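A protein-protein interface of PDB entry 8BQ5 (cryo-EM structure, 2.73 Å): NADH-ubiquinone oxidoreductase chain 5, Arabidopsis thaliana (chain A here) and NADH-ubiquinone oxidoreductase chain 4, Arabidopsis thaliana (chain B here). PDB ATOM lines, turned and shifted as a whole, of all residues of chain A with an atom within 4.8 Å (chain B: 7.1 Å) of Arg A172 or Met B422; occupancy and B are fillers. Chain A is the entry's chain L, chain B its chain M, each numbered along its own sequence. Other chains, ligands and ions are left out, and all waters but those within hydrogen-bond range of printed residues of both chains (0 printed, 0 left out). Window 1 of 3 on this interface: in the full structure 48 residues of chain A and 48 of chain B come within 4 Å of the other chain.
The guanidinium group (NH2) of Arg A172 is in hydrogen-bond range of the backbone carbonyl oxygen (O) of Met B389, at 2.9 Å.
The backbone carbonyl oxygen (O) of Met B422 is in hydrogen-bond range of the guanidinium group (NH1) of Arg A172.
NE of Arg A172 is in salt-bridge range of OE2 of Glu A141 (3.9 Å).
The side-chain carboxylate of Glu A141 lies close to the side-chain carboxylate of Asp A175 (2.7 Å).
CD of Pro B392 touches CG of Glu A141, 3.5 Å away.
Leu A169 touches Ile B423 (CD2 to O, 3.9 Å).
CD2 of Leu A169 touches CA of Ala B427, 3.6 Å away.
Arg A172 touches Ile B423.
Arg A172 touches Ala B426 (NH1 to CB, 3.9 Å).
CG2 of Val A173 touches CD1 of Ile B423 (3.99 Å).
CE of Met B422 touches O of Asp A175, 3.6 Å away.
Ala B419 touches Phe A176.
Phe A176 touches Met B422.
Phe A176 touches Ile B423.
Printed residues of chain B within 4 Å of Glu A141: Pro B392.
Printed residues of chain B within 4 Å of Met A168: Leu B430.
Of chain B, only Met B389 (2.9 Å), Met B422 (2.8 Å), Ile B423 (3.9 Å) and Ala B426 (3.9 Å) come within 4 Å of Arg A172.
Of the printed residues of chain B, Asp A175 touches Met B422 (3.6 Å).
Ile B291 touches none of the printed residues of chain A.
Glu B400 touches none of the printed residues of chain A.
Of the printed residues of chain A, Ala B419 touches Phe A176.
Met B422 touches three residues of chain A.
Of the printed residues of chain A, Leu B430 touches Met A168 (3.6 Å).
The nearest residue of chain A that does not touch Met B422 is Ala A179 (4.1 Å).
Of the 11 printed residues of chain A, 7 touch a printed residue of chain B.
Printed residues of chain A that touch a printed residue of chain B: Glu A141, Met A168, Leu A169, Arg A172, Val A173, Asp A175 and Phe A176.
Hydrophobic or aromatic side chains of chain A that line the printed part of chain B: Met A168, Leu A169, Val A173 and Phe A176.
Along chain A the printed residues that touch a printed residue of chain B span positions 141 to 176.
Hydrophobic or aromatic side chains of chain B that line the printed part of chain A: Met B389, Pro B392, Ala B419, Leu B420, Met B422, Ile B423, Ala B426, Ala B427 and Leu B430.
Among the printed residues, 14 pairs touch across the chains.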
ATOM      1  N   GLU A 141      -7.726 -24.173 -19.391  1.00  0.00           N
ATOM      2  CA  GLU A 141      -8.353 -22.969 -18.854  1.00  0.00           C
ATOM      3  C   GLU A 141      -9.417 -23.310 -17.821  1.00  0.00           C
ATOM      4  O   GLU A 141      -9.667 -22.527 -16.897  1.00  0.00           O
ATOM      5  CB  GLU A 141      -8.969 -22.152 -19.989  1.00  0.00           C
ATOM      6  CG  GLU A 141      -8.040 -21.831 -21.155  1.00  0.00           C
ATOM      7  CD  GLU A 141      -6.848 -20.982 -20.781  1.00  0.00           C
ATOM      8  OE1 GLU A 141      -6.038 -21.414 -19.938  1.00  0.00           O
ATOM      9  OE2 GLU A 141      -6.719 -19.872 -21.338  1.00  0.00           O
ATOM     10  N   MET A 168      -4.907 -16.752 -11.119  1.00  0.00           N
ATOM     11  CA  MET A 168      -5.406 -16.634 -12.485  1.00  0.00           C
ATOM     12  C   MET A 168      -4.410 -15.915 -13.387  1.00  0.00           C
ATOM     13  O   MET A 168      -4.156 -16.343 -14.518  1.00  0.00           O
ATOM     14  CB  MET A 168      -6.748 -15.902 -12.485  1.00  0.00           C
ATOM     15  CG  MET A 168      -7.959 -16.811 -12.514  1.00  0.00           C
ATOM     16  SD  MET A 168      -8.111 -17.754 -14.041  1.00  0.00           S
ATOM     17  CE  MET A 168      -9.874 -17.619 -14.331  1.00  0.00           C
ATOM     18  N   LEU A 169      -3.836 -14.814 -12.900  1.00  0.00           N
ATOM     19  CA  LEU A 169      -2.991 -13.983 -13.752  1.00  0.00           C
ATOM     20  C   LEU A 169      -1.646 -14.640 -14.026  1.00  0.00           C
ATOM     21  O   LEU A 169      -1.120 -14.545 -15.140  1.00  0.00           O
ATOM     22  CB  LEU A 169      -2.800 -12.607 -13.121  1.00  0.00           C
ATOM     23  CG  LEU A 169      -4.061 -11.749 -13.158  1.00  0.00           C
ATOM     24  CD1 LEU A 169      -3.845 -10.429 -12.440  1.00  0.00           C
ATOM     25  CD2 LEU A 169      -4.489 -11.529 -14.596  1.00  0.00           C
ATOM     26  N   VAL A 170      -1.063 -15.293 -13.019  1.00  0.00           N
ATOM     27  CA  VAL A 170       0.190 -16.008 -13.242  1.00  0.00           C
ATOM     28  C   VAL A 170      -0.023 -17.137 -14.239  1.00  0.00           C
ATOM     29  O   VAL A 170       0.794 -17.355 -15.140  1.00  0.00           O
ATOM     30  CB  VAL A 170       0.761 -16.523 -11.908  1.00  0.00           C
ATOM     31  CG1 VAL A 170       2.006 -17.344 -12.154  1.00  0.00           C
ATOM     32  CG2 VAL A 170       1.078 -15.361 -10.984  1.00  0.00           C
ATOM     33  N   ASN A 171      -1.139 -17.858 -14.108  1.00  0.00           N
ATOM     34  CA  ASN A 171      -1.411 -18.969 -15.011  1.00  0.00           C
ATOM     35  C   ASN A 171      -1.830 -18.479 -16.393  1.00  0.00           C
ATOM     36  O   ASN A 171      -1.653 -19.190 -17.387  1.00  0.00           O
ATOM     37  CB  ASN A 171      -2.478 -19.879 -14.409  1.00  0.00           C
ATOM     38  CG  ASN A 171      -1.908 -20.833 -13.373  1.00  0.00           C
ATOM     39  OD1 ASN A 171      -1.192 -21.774 -13.711  1.00  0.00           O
ATOM     40  ND2 ASN A 171      -2.219 -20.589 -12.106  1.00  0.00           N
ATOM     41  N   ARG A 172      -2.388 -17.269 -16.479  1.00  0.00           N
ATOM     42  CA  ARG A 172      -2.725 -16.716 -17.789  1.00  0.00           C
ATOM     43  C   ARG A 172      -1.470 -16.376 -18.579  1.00  0.00           C
ATOM     44  O   ARG A 172      -1.477 -16.404 -19.816  1.00  0.00           O
ATOM     45  CB  ARG A 172      -3.615 -15.482 -17.639  1.00  0.00           C
ATOM     46  CG  ARG A 172      -5.083 -15.773 -17.871  1.00  0.00           C
ATOM     47  CD  ARG A 172      -5.364 -15.960 -19.348  1.00  0.00           C
ATOM     48  NE  ARG A 172      -6.724 -16.422 -19.589  1.00  0.00           N
ATOM     49  CZ  ARG A 172      -7.618 -15.775 -20.322  1.00  0.00           C
ATOM     50  NH1 ARG A 172      -7.324 -14.633 -20.922  1.00  0.00           N
ATOM     51  NH2 ARG A 172      -8.838 -16.287 -20.460  1.00  0.00           N
ATOM     52  N   VAL A 173      -0.384 -16.035 -17.882  1.00  0.00           N
ATOM     53  CA  VAL A 173       0.903 -15.852 -18.548  1.00  0.00           C
ATOM     54  C   VAL A 173       1.380 -17.172 -19.141  1.00  0.00           C
ATOM     55  O   VAL A 173       1.909 -17.215 -20.257  1.00  0.00           O
ATOM     56  CB  VAL A 173       1.931 -15.261 -17.565  1.00  0.00           C
ATOM     57  CG1 VAL A 173       3.327 -15.306 -18.159  1.00  0.00           C
ATOM     58  CG2 VAL A 173       1.551 -13.837 -17.205  1.00  0.00           C
ATOM     59  N   GLY A 174       1.204 -18.267 -18.400  1.00  0.00           N
ATOM     60  CA  GLY A 174       1.499 -19.575 -18.957  1.00  0.00           C
ATOM     61  C   GLY A 174       0.614 -19.913 -20.141  1.00  0.00           C
ATOM     62  O   GLY A 174       1.081 -20.474 -21.135  1.00  0.00           O
ATOM     63  N   ASP A 175      -0.674 -19.571 -20.055  1.00  0.00           N
ATOM     64  CA  ASP A 175      -1.571 -19.781 -21.187  1.00  0.00           C
ATOM     65  C   ASP A 175      -1.130 -18.970 -22.397  1.00  0.00           C
ATOM     66  O   ASP A 175      -1.398 -19.351 -23.542  1.00  0.00           O
ATOM     67  CB  ASP A 175      -3.002 -19.419 -20.796  1.00  0.00           C
ATOM     68  CG  ASP A 175      -3.462 -20.134 -19.548  1.00  0.00           C
ATOM     69  OD1 ASP A 175      -2.956 -21.243 -19.276  1.00  0.00           O
ATOM     70  OD2 ASP A 175      -4.326 -19.586 -18.833  1.00  0.00           O
ATOM     71  N   PHE A 176      -0.468 -17.838 -22.160  1.00  0.00           N
ATOM     72  CA  PHE A 176       0.081 -17.041 -23.253  1.00  0.00           C
ATOM     73  C   PHE A 176       1.154 -17.819 -24.007  1.00  0.00           C
ATOM     74  O   PHE A 176       1.162 -17.853 -25.242  1.00  0.00           O
ATOM     75  CB  PHE A 176       0.621 -15.726 -22.686  1.00  0.00           C
ATOM     76  CG  PHE A 176       1.500 -14.949 -23.625  1.00  0.00           C
ATOM     77  CD1 PHE A 176       0.950 -14.050 -24.522  1.00  0.00           C
ATOM     78  CD2 PHE A 176       2.878 -15.070 -23.566  1.00  0.00           C
ATOM     79  CE1 PHE A 176       1.756 -13.317 -25.369  1.00  0.00           C
ATOM     80  CE2 PHE A 176       3.688 -14.339 -24.410  1.00  0.00           C
ATOM     81  CZ  PHE A 176       3.125 -13.461 -25.313  1.00  0.00           C
ATOM     82  N   ALA A 179      -0.618 -20.917 -25.724  1.00  0.00           N
ATOM     83  CA  ALA A 179      -1.383 -20.534 -26.909  1.00  0.00           C
ATOM     84  C   ALA A 179      -0.469 -20.276 -28.099  1.00  0.00           C
ATOM     85  O   ALA A 179      -0.776 -20.687 -29.223  1.00  0.00           O
ATOM     86  CB  ALA A 179      -2.237 -19.302 -26.615  1.00  0.00           C
ATOM     87  N   ILE B 291      -4.447  -2.278 -28.482  1.00  0.00           N
ATOM     88  CA  ILE B 291      -4.765  -3.393 -27.592  1.00  0.00           C
ATOM     89  C   ILE B 291      -3.991  -3.263 -26.288  1.00  0.00           C
ATOM     90  O   ILE B 291      -4.545  -3.418 -25.196  1.00  0.00           O
ATOM     91  CB  ILE B 291      -4.479  -4.739 -28.278  1.00  0.00           C
ATOM     92  CG1 ILE B 291      -5.487  -5.001 -29.395  1.00  0.00           C
ATOM     93  CG2 ILE B 291      -4.524  -5.871 -27.263  1.00  0.00           C
ATOM     94  CD1 ILE B 291      -5.154  -6.211 -30.233  1.00  0.00           C
ATOM     95  N   LEU B 386     -16.601 -13.950 -17.824  1.00  0.00           N
ATOM     96  CA  LEU B 386     -15.762 -14.977 -18.433  1.00  0.00           C
ATOM     97  C   LEU B 386     -15.739 -14.851 -19.949  1.00  0.00           C
ATOM     98  O   LEU B 386     -14.688 -15.015 -20.578  1.00  0.00           O
ATOM     99  CB  LEU B 386     -16.255 -16.366 -18.036  1.00  0.00           C
ATOM    100  CG  LEU B 386     -16.154 -16.759 -16.568  1.00  0.00           C
ATOM    101  CD1 LEU B 386     -16.661 -18.178 -16.397  1.00  0.00           C
ATOM    102  CD2 LEU B 386     -14.721 -16.625 -16.085  1.00  0.00           C
ATOM    103  N   ASN B 388     -15.931 -12.268 -21.631  1.00  0.00           N
ATOM    104  CA  ASN B 388     -15.118 -11.119 -22.011  1.00  0.00           C
ATOM    105  C   ASN B 388     -13.626 -11.411 -21.910  1.00  0.00           C
ATOM    106  O   ASN B 388     -12.819 -10.643 -22.442  1.00  0.00           O
ATOM    107  CB  ASN B 388     -15.479  -9.909 -21.148  1.00  0.00           C
ATOM    108  CG  ASN B 388     -15.100  -8.592 -21.800  1.00  0.00           C
ATOM    109  OD1 ASN B 388     -14.398  -7.775 -21.209  1.00  0.00           O
ATOM    110  ND2 ASN B 388     -15.574  -8.378 -23.022  1.00  0.00           N
ATOM    111  N   MET B 389     -13.243 -12.498 -21.244  1.00  0.00           N
ATOM    112  CA  MET B 389     -11.851 -12.919 -21.159  1.00  0.00           C
ATOM    113  C   MET B 389     -11.485 -13.953 -22.212  1.00  0.00           C
ATOM    114  O   MET B 389     -10.414 -14.561 -22.112  1.00  0.00           O
ATOM    115  CB  MET B 389     -11.547 -13.491 -19.770  1.00  0.00           C
ATOM    116  CG  MET B 389     -12.136 -12.698 -18.627  1.00  0.00           C
ATOM    117  SD  MET B 389     -12.132 -13.610 -17.073  1.00  0.00           S
ATOM    118  CE  MET B 389     -10.404 -14.001 -16.909  1.00  0.00           C
ATOM    119  N   SER B 390     -12.353 -14.176 -23.200  1.00  0.00           N
ATOM    120  CA  SER B 390     -12.140 -15.182 -24.242  1.00  0.00           C
ATOM    121  C   SER B 390     -11.889 -16.567 -23.652  1.00  0.00           C
ATOM    122  O   SER B 390     -10.944 -17.255 -24.041  1.00  0.00           O
ATOM    123  CB  SER B 390     -10.995 -14.785 -25.177  1.00  0.00           C
ATOM    124  OG  SER B 390     -11.394 -13.745 -26.053  1.00  0.00           O
ATOM    125  N   LEU B 391     -12.718 -16.977 -22.701  1.00  0.00           N
ATOM    126  CA  LEU B 391     -12.575 -18.296 -22.107  1.00  0.00           C
ATOM    127  C   LEU B 391     -13.061 -19.365 -23.085  1.00  0.00           C
ATOM    128  O   LEU B 391     -14.148 -19.219 -23.662  1.00  0.00           O
ATOM    129  CB  LEU B 391     -13.365 -18.383 -20.801  1.00  0.00           C
ATOM    130  CG  LEU B 391     -13.080 -19.597 -19.915  1.00  0.00           C
ATOM    131  CD1 LEU B 391     -11.876 -19.340 -19.024  1.00  0.00           C
ATOM    132  CD2 LEU B 391     -14.301 -19.963 -19.089  1.00  0.00           C
ATOM    133  N   PRO B 392     -12.294 -20.433 -23.305  1.00  0.00           N
ATOM    134  CA  PRO B 392     -12.765 -21.512 -24.181  1.00  0.00           C
ATOM    135  C   PRO B 392     -14.088 -22.076 -23.688  1.00  0.00           C
ATOM    136  O   PRO B 392     -14.303 -22.253 -22.488  1.00  0.00           O
ATOM    137  CB  PRO B 392     -11.641 -22.550 -24.101  1.00  0.00           C
ATOM    138  CG  PRO B 392     -10.435 -21.754 -23.761  1.00  0.00           C
ATOM    139  CD  PRO B 392     -10.912 -20.655 -22.855  1.00  0.00           C
ATOM    140  N   PHE B 397     -13.977 -16.756 -27.461  1.00  0.00           N
ATOM    141  CA  PHE B 397     -12.731 -17.494 -27.642  1.00  0.00           C
ATOM    142  C   PHE B 397     -12.574 -17.969 -29.081  1.00  0.00           C
ATOM    143  O   PHE B 397     -11.457 -18.015 -29.607  1.00  0.00           O
ATOM    144  CB  PHE B 397     -12.661 -18.686 -26.688  1.00  0.00           C
ATOM    145  CG  PHE B 397     -11.516 -19.614 -26.980  1.00  0.00           C
ATOM    146  CD1 PHE B 397     -10.216 -19.237 -26.694  1.00  0.00           C
ATOM    147  CD2 PHE B 397     -11.735 -20.850 -27.568  1.00  0.00           C
ATOM    148  CE1 PHE B 397      -9.159 -20.080 -26.972  1.00  0.00           C
ATOM    149  CE2 PHE B 397     -10.681 -21.697 -27.847  1.00  0.00           C
ATOM    150  CZ  PHE B 397      -9.392 -21.311 -27.548  1.00  0.00           C
ATOM    151  N   GLU B 400     -11.346 -15.110 -31.111  1.00  0.00           N
ATOM    152  CA  GLU B 400     -10.040 -14.645 -30.654  1.00  0.00           C
ATOM    153  C   GLU B 400      -8.920 -15.566 -31.121  1.00  0.00           C
ATOM    154  O   GLU B 400      -7.875 -15.102 -31.589  1.00  0.00           O
ATOM    155  CB  GLU B 400     -10.029 -14.529 -29.131  1.00  0.00           C
ATOM    156  CG  GLU B 400      -8.820 -13.804 -28.584  1.00  0.00           C
ATOM    157  CD  GLU B 400      -7.967 -14.689 -27.700  1.00  0.00           C
ATOM    158  OE1 GLU B 400      -8.316 -15.876 -27.527  1.00  0.00           O
ATOM    159  OE2 GLU B 400      -6.947 -14.195 -27.179  1.00  0.00           O
ATOM    160  N   PHE B 401      -9.111 -16.877 -30.983  1.00  0.00           N
ATOM    161  CA  PHE B 401      -8.042 -17.800 -31.341  1.00  0.00           C
ATOM    162  C   PHE B 401      -7.881 -17.897 -32.851  1.00  0.00           C
ATOM    163  O   PHE B 401      -6.755 -17.938 -33.360  1.00  0.00           O
ATOM    164  CB  PHE B 401      -8.303 -19.176 -30.732  1.00  0.00           C
ATOM    165  CG  PHE B 401      -7.083 -20.042 -30.673  1.00  0.00           C
ATOM    166  CD1 PHE B 401      -6.138 -19.859 -29.678  1.00  0.00           C
ATOM    167  CD2 PHE B 401      -6.869 -21.024 -31.622  1.00  0.00           C
ATOM    168  CE1 PHE B 401      -5.008 -20.647 -29.626  1.00  0.00           C
ATOM    169  CE2 PHE B 401      -5.741 -21.816 -31.574  1.00  0.00           C
ATOM    170  CZ  PHE B 401      -4.810 -21.627 -30.576  1.00  0.00           C
ATOM    171  N   LEU B 404      -5.787 -15.091 -33.935  1.00  0.00           N
ATOM    172  CA  LEU B 404      -4.382 -15.293 -33.593  1.00  0.00           C
ATOM    173  C   LEU B 404      -3.733 -16.310 -34.523  1.00  0.00           C
ATOM    174  O   LEU B 404      -2.547 -16.191 -34.853  1.00  0.00           O
ATOM    175  CB  LEU B 404      -4.251 -15.722 -32.132  1.00  0.00           C
ATOM    176  CG  LEU B 404      -4.580 -14.642 -31.097  1.00  0.00           C
ATOM    177  CD1 LEU B 404      -4.496 -15.194 -29.684  1.00  0.00           C
ATOM    178  CD2 LEU B 404      -3.661 -13.445 -31.260  1.00  0.00           C
ATOM    179  N   LEU B 417       2.168  -9.736 -29.770  1.00  0.00           N
ATOM    180  CA  LEU B 417       1.671  -8.533 -29.114  1.00  0.00           C
ATOM    181  C   LEU B 417       0.160  -8.599 -28.920  1.00  0.00           C
ATOM    182  O   LEU B 417      -0.358  -8.169 -27.883  1.00  0.00           O
ATOM    183  CB  LEU B 417       2.057  -7.296 -29.923  1.00  0.00           C
ATOM    184  CG  LEU B 417       3.547  -7.053 -30.177  1.00  0.00           C
ATOM    185  CD1 LEU B 417       3.726  -5.854 -31.094  1.00  0.00           C
ATOM    186  CD2 LEU B 417       4.322  -6.864 -28.881  1.00  0.00           C
ATOM    187  N   ALA B 418      -0.560  -9.136 -29.909  1.00  0.00           N
ATOM    188  CA  ALA B 418      -2.005  -9.297 -29.780  1.00  0.00           C
ATOM    189  C   ALA B 418      -2.367 -10.309 -28.701  1.00  0.00           C
ATOM    190  O   ALA B 418      -3.366 -10.128 -27.997  1.00  0.00           O
ATOM    191  CB  ALA B 418      -2.612  -9.717 -31.118  1.00  0.00           C
ATOM    192  N   ALA B 419      -1.581 -11.377 -28.559  1.00  0.00           N
ATOM    193  CA  ALA B 419      -1.873 -12.384 -27.546  1.00  0.00           C
ATOM    194  C   ALA B 419      -1.695 -11.852 -26.130  1.00  0.00           C
ATOM    195  O   ALA B 419      -2.139 -12.500 -25.179  1.00  0.00           O
ATOM    196  CB  ALA B 419      -0.999 -13.618 -27.756  1.00  0.00           C
ATOM    197  N   LEU B 420      -1.056 -10.689 -25.969  1.00  0.00           N
ATOM    198  CA  LEU B 420      -0.976 -10.064 -24.654  1.00  0.00           C
ATOM    199  C   LEU B 420      -2.339  -9.587 -24.176  1.00  0.00           C
ATOM    200  O   LEU B 420      -2.500  -9.245 -22.999  1.00  0.00           O
ATOM    201  CB  LEU B 420       0.011  -8.899 -24.680  1.00  0.00           C
ATOM    202  CG  LEU B 420       1.476  -9.273 -24.886  1.00  0.00           C
ATOM    203  CD1 LEU B 420       2.303  -8.031 -25.153  1.00  0.00           C
ATOM    204  CD2 LEU B 420       2.001 -10.019 -23.674  1.00  0.00           C
ATOM    205  N   GLY B 421      -3.327  -9.545 -25.069  1.00  0.00           N
ATOM    206  CA  GLY B 421      -4.679  -9.236 -24.642  1.00  0.00           C
ATOM    207  C   GLY B 421      -5.242 -10.277 -23.696  1.00  0.00           C
ATOM    208  O   GLY B 421      -6.126  -9.984 -22.889  1.00  0.00           O
ATOM    209  N   MET B 422      -4.744 -11.514 -23.789  1.00  0.00           N
ATOM    210  CA  MET B 422      -5.194 -12.566 -22.881  1.00  0.00           C
ATOM    211  C   MET B 422      -4.798 -12.264 -21.442  1.00  0.00           C
ATOM    212  O   MET B 422      -5.597 -12.450 -20.518  1.00  0.00           O
ATOM    213  CB  MET B 422      -4.628 -13.919 -23.320  1.00  0.00           C
ATOM    214  CG  MET B 422      -4.813 -14.222 -24.799  1.00  0.00           C
ATOM    215  SD  MET B 422      -3.878 -15.651 -25.391  1.00  0.00           S
ATOM    216  CE  MET B 422      -3.580 -16.546 -23.870  1.00  0.00           C
ATOM    217  N   ILE B 423      -3.565 -11.805 -21.230  1.00  0.00           N
ATOM    218  CA  ILE B 423      -3.122 -11.473 -19.880  1.00  0.00           C
ATOM    219  C   ILE B 423      -3.848 -10.239 -19.361  1.00  0.00           C
ATOM    220  O   ILE B 423      -4.362 -10.234 -18.237  1.00  0.00           O
ATOM    221  CB  ILE B 423      -1.597 -11.274 -19.856  1.00  0.00           C
ATOM    222  CG1 ILE B 423      -0.878 -12.588 -20.152  1.00  0.00           C
ATOM    223  CG2 ILE B 423      -1.154 -10.735 -18.507  1.00  0.00           C
ATOM    224  CD1 ILE B 423       0.482 -12.396 -20.773  1.00  0.00           C
ATOM    225  N   LEU B 424      -3.908  -9.181 -20.172  1.00  0.00           N
ATOM    226  CA  LEU B 424      -4.478  -7.920 -19.712  1.00  0.00           C
ATOM    227  C   LEU B 424      -5.998  -7.992 -19.635  1.00  0.00           C
ATOM    228  O   LEU B 424      -6.603  -7.458 -18.699  1.00  0.00           O
ATOM    229  CB  LEU B 424      -4.035  -6.786 -20.635  1.00  0.00           C
ATOM    230  CG  LEU B 424      -2.531  -6.510 -20.710  1.00  0.00           C
ATOM    231  CD1 LEU B 424      -2.238  -5.390 -21.696  1.00  0.00           C
ATOM    232  CD2 LEU B 424      -1.968  -6.179 -19.338  1.00  0.00           C
ATOM    233  N   GLY B 425      -6.630  -8.649 -20.609  1.00  0.00           N
ATOM    234  CA  GLY B 425      -8.080  -8.769 -20.590  1.00  0.00           C
ATOM    235  C   GLY B 425      -8.593  -9.514 -19.374  1.00  0.00           C
ATOM    236  O   GLY B 425      -9.662  -9.199 -18.846  1.00  0.00           O
ATOM    237  N   ALA B 426      -7.840 -10.512 -18.914  1.00  0.00           N
ATOM    238  CA  ALA B 426      -8.240 -11.262 -17.730  1.00  0.00           C
ATOM    239  C   ALA B 426      -8.036 -10.439 -16.465  1.00  0.00           C
ATOM    240  O   ALA B 426      -8.749 -10.617 -15.470  1.00  0.00           O
ATOM    241  CB  ALA B 426      -7.449 -12.568 -17.656  1.00  0.00           C
ATOM    242  N   ALA B 427      -7.055  -9.537 -16.483  1.00  0.00           N
ATOM    243  CA  ALA B 427      -6.722  -8.778 -15.283  1.00  0.00           C
ATOM    244  C   ALA B 427      -7.850  -7.835 -14.886  1.00  0.00           C
ATOM    245  O   ALA B 427      -8.299  -7.836 -13.735  1.00  0.00           O
ATOM    246  CB  ALA B 427      -5.422  -8.004 -15.499  1.00  0.00           C
ATOM    247  N   LEU B 430     -11.522  -9.731 -14.195  1.00  0.00           N
ATOM    248  CA  LEU B 430     -11.656 -10.343 -12.879  1.00  0.00           C
ATOM    249  C   LEU B 430     -11.616  -9.293 -11.778  1.00  0.00           C
ATOM    250  O   LEU B 430     -12.321  -9.419 -10.771  1.00  0.00           O
ATOM    251  CB  LEU B 430     -10.559 -11.384 -12.669  1.00  0.00           C
ATOM    252  CG  LEU B 430     -10.715 -12.690 -13.447  1.00  0.00           C
ATOM    253  CD1 LEU B 430      -9.555 -13.612 -13.140  1.00  0.00           C
ATOM    254  CD2 LEU B 430     -12.038 -13.362 -13.125  1.00  0.00           C
